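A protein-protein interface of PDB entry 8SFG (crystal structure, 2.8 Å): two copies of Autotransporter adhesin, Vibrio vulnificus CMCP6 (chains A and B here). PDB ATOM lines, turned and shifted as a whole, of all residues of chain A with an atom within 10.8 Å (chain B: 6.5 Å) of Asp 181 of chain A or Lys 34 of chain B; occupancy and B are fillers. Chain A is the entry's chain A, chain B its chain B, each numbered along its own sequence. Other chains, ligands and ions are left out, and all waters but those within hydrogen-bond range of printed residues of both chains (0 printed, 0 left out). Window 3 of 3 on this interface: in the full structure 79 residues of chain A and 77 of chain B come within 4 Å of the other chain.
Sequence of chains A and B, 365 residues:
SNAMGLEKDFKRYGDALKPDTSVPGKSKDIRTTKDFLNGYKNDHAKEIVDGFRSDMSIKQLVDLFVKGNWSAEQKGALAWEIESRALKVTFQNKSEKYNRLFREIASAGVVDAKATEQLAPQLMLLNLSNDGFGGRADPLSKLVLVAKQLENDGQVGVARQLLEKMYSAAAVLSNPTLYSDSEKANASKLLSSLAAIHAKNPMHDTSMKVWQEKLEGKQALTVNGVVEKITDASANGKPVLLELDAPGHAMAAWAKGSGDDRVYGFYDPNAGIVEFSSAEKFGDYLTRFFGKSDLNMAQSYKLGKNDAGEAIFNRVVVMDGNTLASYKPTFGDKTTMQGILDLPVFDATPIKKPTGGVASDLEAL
Of the 10 printed residues of chain B, 4 touch a printed residue of chain A.
Hydrophobic or aromatic side chains of chain B that line the printed part of chain A: Leu 37 and Tyr 40.
Along chain B the printed residues that touch a printed residue of chain A span positions 34 to 40.
Of the 21 printed residues of chain A, 5 touch a printed residue of chain B.
Hydrophobic or aromatic side chains of chain A that line the printed part of chain B: Leu 173 and Pro 176.
The side-chain amino group of Lys 184 of chain A is in salt-bridge range of the side-chain carboxylate of Asp 181 of chain A (3.7 Å).
O of Lys 184 of chain A lies within hydrogen-bond range of OG of Ser 188 of chain A (3.3 Å).
The backbone carbonyl oxygen of Ala 185 of chain A is in hydrogen-bond range of the side-chain hydroxyl of Ser 188 of chain A (2.9 Å).
OD1 of Asn 38 of chain B sits close to O of Lys 34 of chain B (3.2 Å).
Ser 180 of chain A touches none of the printed residues of chain B.
Asp 181 of chain A touches just these residues of chain B: Lys 34 (3.7 Å), Leu 37 (3.5 Å) and Asn 38 (3.0 Å).
Of the printed residues of chain B, Lys 184 of chain A touches Leu 37 and Tyr 40.
Printed residues of chain B within 4 Å of Ser 188 of chain A: Tyr 40.
No residue of chain A comes within 4 Å of Thr 33 of chain B.
Lys 34 of chain B touches just one residue of chain A: Asp 181.
No residue of chain A comes within 4 Å of Asp 35 of chain B.
Phe 36 of chain B touches none of the printed residues of chain A.
Printed residues of chain A within 4 Å of Leu 37 of chain B: Asp 181 (3.5 Å) and Lys 184 (2.6 Å).
Asn 38 of chain B touches one residue of chain A.
No position is printed for both chains.
The side-chain amide oxygen of Asn 38 of chain B lies close to the side-chain carboxylate of Asp 181 of chain A (3.0 Å).
The side-chain amino group (NZ) of Lys 184 of chain A is in hydrogen-bond range of the backbone carbonyl oxygen (O) of Leu 37 of chain B (2.6 Å).
O of Tyr 40 of chain B sits at hydrogen-bond distance from NZ of Lys 184 of chain A, 2.8 Å away.
Tyr 40 of chain B touches Leu 173 of chain A.
Tyr 40 of chain B touches Pro 176 of chain A (O to CB, 3.97 Å).
Lys 34 of chain B touches Asp 181 of chain A.
Asp 181 of chain A touches Leu 37 of chain B.
CB of Ser 188 of chain A touches OH of Tyr 40 of chain B, 3.7 Å away.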
ATOM      1  N   VAL A 172      -9.731  34.845 -28.766  1.00  0.00           N
ATOM      2  CA  VAL A 172     -10.249  33.505 -29.177  1.00  0.00           C
ATOM      3  C   VAL A 172     -11.179  32.974 -28.082  1.00  0.00           C
ATOM      4  O   VAL A 172     -12.218  32.379 -28.422  1.00  0.00           O
ATOM      5  CB  VAL A 172      -9.097  32.522 -29.473  1.00  0.00           C
ATOM      6  CG1 VAL A 172      -9.591  31.099 -29.656  1.00  0.00           C
ATOM      7  CG2 VAL A 172      -8.278  32.963 -30.679  1.00  0.00           C
ATOM      8  N   LEU A 173     -10.819  33.206 -26.820  1.00  0.00           N
ATOM      9  CA  LEU A 173     -11.626  32.732 -25.662  1.00  0.00           C
ATOM     10  C   LEU A 173     -12.946  33.520 -25.583  1.00  0.00           C
ATOM     11  O   LEU A 173     -13.929  32.943 -25.098  1.00  0.00           O
ATOM     12  CB  LEU A 173     -10.778  32.906 -24.396  1.00  0.00           C
ATOM     13  CG  LEU A 173     -11.371  32.393 -23.090  1.00  0.00           C
ATOM     14  CD1 LEU A 173     -11.664  30.905 -23.178  1.00  0.00           C
ATOM     15  CD2 LEU A 173     -10.423  32.685 -21.935  1.00  0.00           C
ATOM     16  N   ASN A 175     -14.578  34.961 -28.337  1.00  0.00           N
ATOM     17  CA  ASN A 175     -15.380  34.692 -29.564  1.00  0.00           C
ATOM     18  C   ASN A 175     -14.912  33.384 -30.194  1.00  0.00           C
ATOM     19  O   ASN A 175     -14.438  33.375 -31.327  1.00  0.00           O
ATOM     20  CB  ASN A 175     -15.249  35.855 -30.551  1.00  0.00           C
ATOM     21  CG  ASN A 175     -15.756  37.168 -29.991  1.00  0.00           C
ATOM     22  OD1 ASN A 175     -15.056  38.179 -30.029  1.00  0.00           O
ATOM     23  ND2 ASN A 175     -16.948  37.151 -29.417  1.00  0.00           N
ATOM     24  N   PRO A 176     -15.073  32.235 -29.500  1.00  0.00           N
ATOM     25  CA  PRO A 176     -14.615  30.947 -30.021  1.00  0.00           C
ATOM     26  C   PRO A 176     -15.293  30.516 -31.329  1.00  0.00           C
ATOM     27  O   PRO A 176     -14.674  29.798 -32.084  1.00  0.00           O
ATOM     28  CB  PRO A 176     -14.959  29.958 -28.894  1.00  0.00           C
ATOM     29  CG  PRO A 176     -16.090  30.634 -28.147  1.00  0.00           C
ATOM     30  CD  PRO A 176     -15.742  32.106 -28.196  1.00  0.00           C
ATOM     31  N   THR A 177     -16.522  30.977 -31.561  1.00  0.00           N
ATOM     32  CA  THR A 177     -17.287  30.605 -32.786  1.00  0.00           C
ATOM     33  C   THR A 177     -16.598  31.140 -34.049  1.00  0.00           C
ATOM     34  O   THR A 177     -16.981  30.694 -35.145  1.00  0.00           O
ATOM     35  CB  THR A 177     -18.735  31.091 -32.692  1.00  0.00           C
ATOM     36  OG1 THR A 177     -18.690  32.483 -32.380  1.00  0.00           O
ATOM     37  CG2 THR A 177     -19.537  30.366 -31.633  1.00  0.00           C
ATOM     38  N   LEU A 178     -15.615  32.037 -33.901  1.00  0.00           N
ATOM     39  CA  LEU A 178     -14.885  32.625 -35.064  1.00  0.00           C
ATOM     40  C   LEU A 178     -13.533  31.932 -35.272  1.00  0.00           C
ATOM     41  O   LEU A 178     -12.779  32.402 -36.145  1.00  0.00           O
ATOM     42  CB  LEU A 178     -14.663  34.124 -34.825  1.00  0.00           C
ATOM     43  CG  LEU A 178     -15.926  34.981 -34.712  1.00  0.00           C
ATOM     44  CD1 LEU A 178     -15.585  36.411 -34.319  1.00  0.00           C
ATOM     45  CD2 LEU A 178     -16.712  34.965 -36.015  1.00  0.00           C
ATOM     46  N   TYR A 179     -13.238  30.860 -34.526  1.00  0.00           N
ATOM     47  CA  TYR A 179     -11.916  30.193 -34.684  1.00  0.00           C
ATOM     48  C   TYR A 179     -12.071  28.671 -34.743  1.00  0.00           C
ATOM     49  O   TYR A 179     -13.101  28.141 -34.309  1.00  0.00           O
ATOM     50  CB  TYR A 179     -10.992  30.632 -33.545  1.00  0.00           C
ATOM     51  CG  TYR A 179     -10.854  32.129 -33.438  1.00  0.00           C
ATOM     52  CD1 TYR A 179      -9.951  32.815 -34.226  1.00  0.00           C
ATOM     53  CD2 TYR A 179     -11.649  32.862 -32.576  1.00  0.00           C
ATOM     54  CE1 TYR A 179      -9.829  34.191 -34.151  1.00  0.00           C
ATOM     55  CE2 TYR A 179     -11.541  34.240 -32.490  1.00  0.00           C
ATOM     56  CZ  TYR A 179     -10.621  34.909 -33.281  1.00  0.00           C
ATOM     57  OH  TYR A 179     -10.465  36.264 -33.256  1.00  0.00           O
ATOM     58  N   SER A 180     -11.044  28.000 -35.269  1.00  0.00           N
ATOM     59  CA  SER A 180     -11.026  26.521 -35.411  1.00  0.00           C
ATOM     60  C   SER A 180     -10.796  25.856 -34.049  1.00  0.00           C
ATOM     61  O   SER A 180     -10.388  26.558 -33.103  1.00  0.00           O
ATOM     62  CB  SER A 180      -9.972  26.102 -36.401  1.00  0.00           C
ATOM     63  OG  SER A 180      -8.681  26.512 -35.970  1.00  0.00           O
ATOM     64  N   ASP A 181     -11.048  24.546 -33.968  1.00  0.00           N
ATOM     65  CA  ASP A 181     -10.849  23.765 -32.718  1.00  0.00           C
ATOM     66  C   ASP A 181      -9.372  23.828 -32.315  1.00  0.00           C
ATOM     67  O   ASP A 181      -9.090  23.919 -31.105  1.00  0.00           O
ATOM     68  CB  ASP A 181     -11.305  22.315 -32.897  1.00  0.00           C
ATOM     69  CG  ASP A 181     -12.795  22.158 -33.145  1.00  0.00           C
ATOM     70  OD1 ASP A 181     -13.509  23.175 -33.073  1.00  0.00           O
ATOM     71  OD2 ASP A 181     -13.224  21.021 -33.408  1.00  0.00           O
ATOM     72  N   SER A 182      -8.475  23.777 -33.306  1.00  0.00           N
ATOM     73  CA  SER A 182      -7.009  23.831 -33.069  1.00  0.00           C
ATOM     74  C   SER A 182      -6.647  25.157 -32.388  1.00  0.00           C
ATOM     75  O   SER A 182      -5.821  25.140 -31.459  1.00  0.00           O
ATOM     76  CB  SER A 182      -6.256  23.671 -34.363  1.00  0.00           C
ATOM     77  OG  SER A 182      -6.673  22.504 -35.057  1.00  0.00           O
ATOM     78  N   GLU A 183      -7.263  26.256 -32.838  1.00  0.00           N
ATOM     79  CA  GLU A 183      -7.011  27.622 -32.299  1.00  0.00           C
ATOM     80  C   GLU A 183      -7.594  27.742 -30.885  1.00  0.00           C
ATOM     81  O   GLU A 183      -6.919  28.348 -30.023  1.00  0.00           O
ATOM     82  CB  GLU A 183      -7.577  28.666 -33.263  1.00  0.00           C
ATOM     83  CG  GLU A 183      -6.814  28.735 -34.578  1.00  0.00           C
ATOM     84  CD  GLU A 183      -7.444  29.579 -35.672  1.00  0.00           C
ATOM     85  OE1 GLU A 183      -8.674  29.733 -35.664  1.00  0.00           O
ATOM     86  OE2 GLU A 183      -6.697  30.081 -36.532  1.00  0.00           O
ATOM     87  N   LYS A 184      -8.788  27.185 -30.655  1.00  0.00           N
ATOM     88  CA  LYS A 184      -9.426  27.247 -29.312  1.00  0.00           C
ATOM     89  C   LYS A 184      -8.586  26.435 -28.317  1.00  0.00           C
ATOM     90  O   LYS A 184      -8.508  26.841 -27.133  1.00  0.00           O
ATOM     91  CB  LYS A 184     -10.875  26.757 -29.375  1.00  0.00           C
ATOM     92  CG  LYS A 184     -11.811  27.627 -30.206  1.00  0.00           C
ATOM     93  CD  LYS A 184     -13.264  27.213 -30.142  1.00  0.00           C
ATOM     94  CE  LYS A 184     -13.520  25.806 -30.638  1.00  0.00           C
ATOM     95  NZ  LYS A 184     -14.957  25.461 -30.556  1.00  0.00           N
ATOM     96  N   ALA A 185      -7.974  25.342 -28.787  1.00  0.00           N
ATOM     97  CA  ALA A 185      -7.126  24.478 -27.933  1.00  0.00           C
ATOM     98  C   ALA A 185      -5.826  25.216 -27.578  1.00  0.00           C
ATOM     99  O   ALA A 185      -5.383  25.106 -26.422  1.00  0.00           O
ATOM    100  CB  ALA A 185      -6.840  23.176 -28.639  1.00  0.00           C
ATOM    101  N   ASN A 186      -5.249  25.940 -28.541  1.00  0.00           N
ATOM    102  CA  ASN A 186      -3.985  26.695 -28.323  1.00  0.00           C
ATOM    103  C   ASN A 186      -4.226  27.848 -27.344  1.00  0.00           C
ATOM    104  O   ASN A 186      -3.377  28.046 -26.453  1.00  0.00           O
ATOM    105  CB  ASN A 186      -3.412  27.230 -29.635  1.00  0.00           C
ATOM    106  CG  ASN A 186      -3.032  26.135 -30.610  1.00  0.00           C
ATOM    107  OD1 ASN A 186      -3.064  24.953 -30.273  1.00  0.00           O
ATOM    108  ND2 ASN A 186      -2.659  26.520 -31.819  1.00  0.00           N
ATOM    109  N   ALA A 187      -5.337  28.573 -27.516  1.00  0.00           N
ATOM    110  CA  ALA A 187      -5.681  29.716 -26.636  1.00  0.00           C
ATOM    111  C   ALA A 187      -5.846  29.229 -25.191  1.00  0.00           C
ATOM    112  O   ALA A 187      -5.276  29.862 -24.284  1.00  0.00           O
ATOM    113  CB  ALA A 187      -6.936  30.398 -27.138  1.00  0.00           C
ATOM    114  N   SER A 188      -6.603  28.148 -24.991  1.00  0.00           N
ATOM    115  CA  SER A 188      -6.817  27.607 -23.623  1.00  0.00           C
ATOM    116  C   SER A 188      -5.487  27.108 -23.043  1.00  0.00           C
ATOM    117  O   SER A 188      -5.252  27.307 -21.845  1.00  0.00           O
ATOM    118  CB  SER A 188      -7.841  26.512 -23.624  1.00  0.00           C
ATOM    119  OG  SER A 188      -7.387  25.417 -24.396  1.00  0.00           O
ATOM    120  N   LYS A 189      -4.638  26.506 -23.879  1.00  0.00           N
ATOM    121  CA  LYS A 189      -3.334  25.974 -23.396  1.00  0.00           C
ATOM    122  C   LYS A 189      -2.450  27.131 -22.918  1.00  0.00           C
ATOM    123  O   LYS A 189      -1.931  27.033 -21.795  1.00  0.00           O
ATOM    124  CB  LYS A 189      -2.654  25.146 -24.489  1.00  0.00           C
ATOM    125  CG  LYS A 189      -1.378  24.429 -24.073  1.00  0.00           C
ATOM    126  CD  LYS A 189      -0.894  23.451 -25.126  1.00  0.00           C
ATOM    127  CE  LYS A 189       0.351  22.688 -24.724  1.00  0.00           C
ATOM    128  NZ  LYS A 189       0.738  21.700 -25.760  1.00  0.00           N
ATOM    129  N   PRO A 344       2.039  28.321 -29.644  1.00  0.00           N
ATOM    130  CA  PRO A 344       1.332  29.004 -30.723  1.00  0.00           C
ATOM    131  C   PRO A 344      -0.136  29.295 -30.383  1.00  0.00           C
ATOM    132  O   PRO A 344      -0.638  28.773 -29.397  1.00  0.00           O
ATOM    133  CB  PRO A 344       1.412  27.958 -31.841  1.00  0.00           C
ATOM    134  CG  PRO A 344       1.252  26.643 -31.098  1.00  0.00           C
ATOM    135  CD  PRO A 344       2.011  26.856 -29.803  1.00  0.00           C
ATOM    136  N   VAL A 345      -0.772  30.132 -31.201  1.00  0.00           N
ATOM    137  CA  VAL A 345      -2.210  30.475 -31.017  1.00  0.00           C
ATOM    138  C   VAL A 345      -2.899  30.211 -32.356  1.00  0.00           C
ATOM    139  O   VAL A 345      -4.015  29.665 -32.332  1.00  0.00           O
ATOM    140  CB  VAL A 345      -2.418  31.925 -30.529  1.00  0.00           C
ATOM    141  CG1 VAL A 345      -3.890  32.308 -30.509  1.00  0.00           C
ATOM    142  CG2 VAL A 345      -1.794  32.157 -29.158  1.00  0.00           C
ATOM    143  N   PHE A 346      -2.228  30.541 -33.469  1.00  0.00           N
ATOM    144  CA  PHE A 346      -2.826  30.337 -34.818  1.00  0.00           C
ATOM    145  C   PHE A 346      -2.044  29.313 -35.652  1.00  0.00           C
ATOM    146  O   PHE A 346      -0.823  29.161 -35.484  1.00  0.00           O
ATOM    147  CB  PHE A 346      -2.991  31.679 -35.537  1.00  0.00           C
ATOM    148  CG  PHE A 346      -3.919  32.630 -34.826  1.00  0.00           C
ATOM    149  CD1 PHE A 346      -5.275  32.355 -34.745  1.00  0.00           C
ATOM    150  CD2 PHE A 346      -3.456  33.816 -34.278  1.00  0.00           C
ATOM    151  CE1 PHE A 346      -6.138  33.216 -34.093  1.00  0.00           C
ATOM    152  CE2 PHE A 346      -4.326  34.687 -33.638  1.00  0.00           C
ATOM    153  CZ  PHE A 346      -5.665  34.385 -33.545  1.00  0.00           C
ATOM    154  N   ASP A 347      -2.790  28.624 -36.522  1.00  0.00           N
ATOM    155  CA  ASP A 347      -2.285  27.572 -37.443  1.00  0.00           C
ATOM    156  C   ASP A 347      -3.425  27.227 -38.414  1.00  0.00           C
ATOM    157  O   ASP A 347      -4.529  27.776 -38.339  1.00  0.00           O
ATOM    158  CB  ASP A 347      -1.769  26.356 -36.660  1.00  0.00           C
ATOM    159  CG  ASP A 347      -1.358  25.166 -37.518  1.00  0.00           C
ATOM    160  OD1 ASP A 347      -1.638  25.186 -38.737  1.00  0.00           O
ATOM    161  OD2 ASP A 347      -0.762  24.223 -36.959  1.00  0.00           O
ATOM    162  N   ILE B  30      -8.998  14.324 -23.436  1.00  0.00           N
ATOM    163  CA  ILE B  30     -10.402  14.692 -23.795  1.00  0.00           C
ATOM    164  C   ILE B  30     -10.451  16.159 -24.248  1.00  0.00           C
ATOM    165  O   ILE B  30     -11.340  16.490 -25.064  1.00  0.00           O
ATOM    166  CB  ILE B  30     -11.371  14.430 -22.621  1.00  0.00           C
ATOM    167  CG1 ILE B  30     -12.838  14.612 -23.032  1.00  0.00           C
ATOM    168  CG2 ILE B  30     -11.019  15.292 -21.418  1.00  0.00           C
ATOM    169  CD1 ILE B  30     -13.309  13.664 -24.113  1.00  0.00           C
ATOM    170  N   THR B  32      -8.656  17.562 -26.278  1.00  0.00           N
ATOM    171  CA  THR B  32      -8.201  17.673 -27.696  1.00  0.00           C
ATOM    172  C   THR B  32      -9.128  16.886 -28.638  1.00  0.00           C
ATOM    173  O   THR B  32      -8.847  16.887 -29.855  1.00  0.00           O
ATOM    174  CB  THR B  32      -6.744  17.215 -27.842  1.00  0.00           C
ATOM    175  OG1 THR B  32      -6.678  15.854 -27.414  1.00  0.00           O
ATOM    176  CG2 THR B  32      -5.775  18.054 -27.037  1.00  0.00           C
ATOM    177  N   THR B  33     -10.186  16.253 -28.112  1.00  0.00           N
ATOM    178  CA  THR B  33     -11.134  15.485 -28.969  1.00  0.00           C
ATOM    179  C   THR B  33     -12.066  16.470 -29.684  1.00  0.00           C
ATOM    180  O   THR B  33     -12.506  17.438 -29.032  1.00  0.00           O
ATOM    181  CB  THR B  33     -11.935  14.455 -28.162  1.00  0.00           C
ATOM    182  OG1 THR B  33     -12.701  15.153 -27.177  1.00  0.00           O
ATOM    183  CG2 THR B  33     -11.061  13.414 -27.500  1.00  0.00           C
ATOM    184  N   LYS B  34     -12.365  16.215 -30.961  1.00  0.00           N
ATOM    185  CA  LYS B  34     -13.249  17.105 -31.767  1.00  0.00           C
ATOM    186  C   LYS B  34     -14.661  17.142 -31.163  1.00  0.00           C
ATOM    187  O   LYS B  34     -15.404  18.092 -31.475  1.00  0.00           O
ATOM    188  CB  LYS B  34     -13.268  16.653 -33.232  1.00  0.00           C
ATOM    189  CG  LYS B  34     -11.911  16.645 -33.928  1.00  0.00           C
ATOM    190  CD  LYS B  34     -11.227  18.004 -33.972  1.00  0.00           C
ATOM    191  CE  LYS B  34      -9.850  17.966 -34.599  1.00  0.00           C
ATOM    192  NZ  LYS B  34      -9.891  17.504 -36.006  1.00  0.00           N
ATOM    193  N   ASP B  35     -15.010  16.156 -30.329  1.00  0.00           N
ATOM    194  CA  ASP B  35     -16.353  16.117 -29.686  1.00  0.00           C
ATOM    195  C   ASP B  35     -16.401  17.171 -28.571  1.00  0.00           C
ATOM    196  O   ASP B  35     -17.453  17.823 -28.412  1.00  0.00           O
ATOM    197  CB  ASP B  35     -16.674  14.725 -29.131  1.00  0.00           C
ATOM    198  CG  ASP B  35     -16.742  13.629 -30.179  1.00  0.00           C
ATOM    199  OD1 ASP B  35     -16.689  13.957 -31.378  1.00  0.00           O
ATOM    200  OD2 ASP B  35     -16.841  12.453 -29.783  1.00  0.00           O
ATOM    201  N   PHE B  36     -15.292  17.321 -27.840  1.00  0.00           N
ATOM    202  CA  PHE B  36     -15.165  18.292 -26.721  1.00  0.00           C
ATOM    203  C   PHE B  36     -15.065  19.723 -27.267  1.00  0.00           C
ATOM    204  O   PHE B  36     -15.821  20.601 -26.809  1.00  0.00           O
ATOM    205  CB  PHE B  36     -13.927  17.948 -25.885  1.00  0.00           C
ATOM    206  CG  PHE B  36     -13.660  18.847 -24.702  1.00  0.00           C
ATOM    207  CD1 PHE B  36     -14.221  18.571 -23.464  1.00  0.00           C
ATOM    208  CD2 PHE B  36     -12.821  19.947 -24.815  1.00  0.00           C
ATOM    209  CE1 PHE B  36     -13.969  19.390 -22.373  1.00  0.00           C
ATOM    210  CE2 PHE B  36     -12.573  20.765 -23.722  1.00  0.00           C
ATOM    211  CZ  PHE B  36     -13.147  20.485 -22.503  1.00  0.00           C
ATOM    212  N   LEU B  37     -14.165  19.929 -28.232  1.00  0.00           N
ATOM    213  CA  LEU B  37     -13.907  21.263 -28.838  1.00  0.00           C
ATOM    214  C   LEU B  37     -15.155  21.818 -29.538  1.00  0.00           C
ATOM    215  O   LEU B  37     -15.315  23.053 -29.515  1.00  0.00           O
ATOM    216  CB  LEU B  37     -12.708  21.138 -29.787  1.00  0.00           C
ATOM    217  CG  LEU B  37     -11.396  20.743 -29.105  1.00  0.00           C
ATOM    218  CD1 LEU B  37     -10.292  20.476 -30.113  1.00  0.00           C
ATOM    219  CD2 LEU B  37     -10.954  21.811 -28.112  1.00  0.00           C
ATOM    220  N   ASN B  38     -15.998  20.964 -30.137  1.00  0.00           N
ATOM    221  CA  ASN B  38     -17.228  21.480 -30.806  1.00  0.00           C
ATOM    222  C   ASN B  38     -18.161  22.081 -29.748  1.00  0.00           C
ATOM    223  O   ASN B  38     -18.843  23.083 -30.062  1.00  0.00           O
ATOM    224  CB  ASN B  38     -17.949  20.422 -31.645  1.00  0.00           C
ATOM    225  CG  ASN B  38     -17.222  20.077 -32.927  1.00  0.00           C
ATOM    226  OD1 ASN B  38     -16.176  20.648 -33.231  1.00  0.00           O
ATOM    227  ND2 ASN B  38     -17.779  19.157 -33.699  1.00  0.00           N
ATOM    228  N   GLY B  39     -18.184  21.491 -28.547  1.00  0.00           N
ATOM    229  CA  GLY B  39     -19.033  21.998 -27.452  1.00  0.00           C
ATOM    230  C   GLY B  39     -18.394  23.194 -26.765  1.00  0.00           C
ATOM    231  O   GLY B  39     -19.125  23.943 -26.082  1.00  0.00           O
ATOM    232  N   TYR B  40     -17.079  23.370 -26.953  1.00  0.00           N
ATOM    233  CA  TYR B  40     -16.308  24.484 -26.337  1.00  0.00           C
ATOM    234  C   TYR B  40     -16.607  25.780 -27.106  1.00  0.00           C
ATOM    235  O   TYR B  40     -15.787  26.186 -27.955  1.00  0.00           O
ATOM    236  CB  TYR B  40     -14.819  24.114 -26.293  1.00  0.00           C
ATOM    237  CG  TYR B  40     -13.923  25.060 -25.531  1.00  0.00           C
ATOM    238  CD1 TYR B  40     -13.776  24.950 -24.156  1.00  0.00           C
ATOM    239  CD2 TYR B  40     -13.184  26.038 -26.180  1.00  0.00           C
ATOM    240  CE1 TYR B  40     -12.947  25.804 -23.444  1.00  0.00           C
ATOM    241  CE2 TYR B  40     -12.352  26.902 -25.485  1.00  0.00           C
ATOM    242  CZ  TYR B  40     -12.231  26.783 -24.112  1.00  0.00           C
ATOM    243  OH  TYR B  40     -11.406  27.627 -23.426  1.00  0.00           O
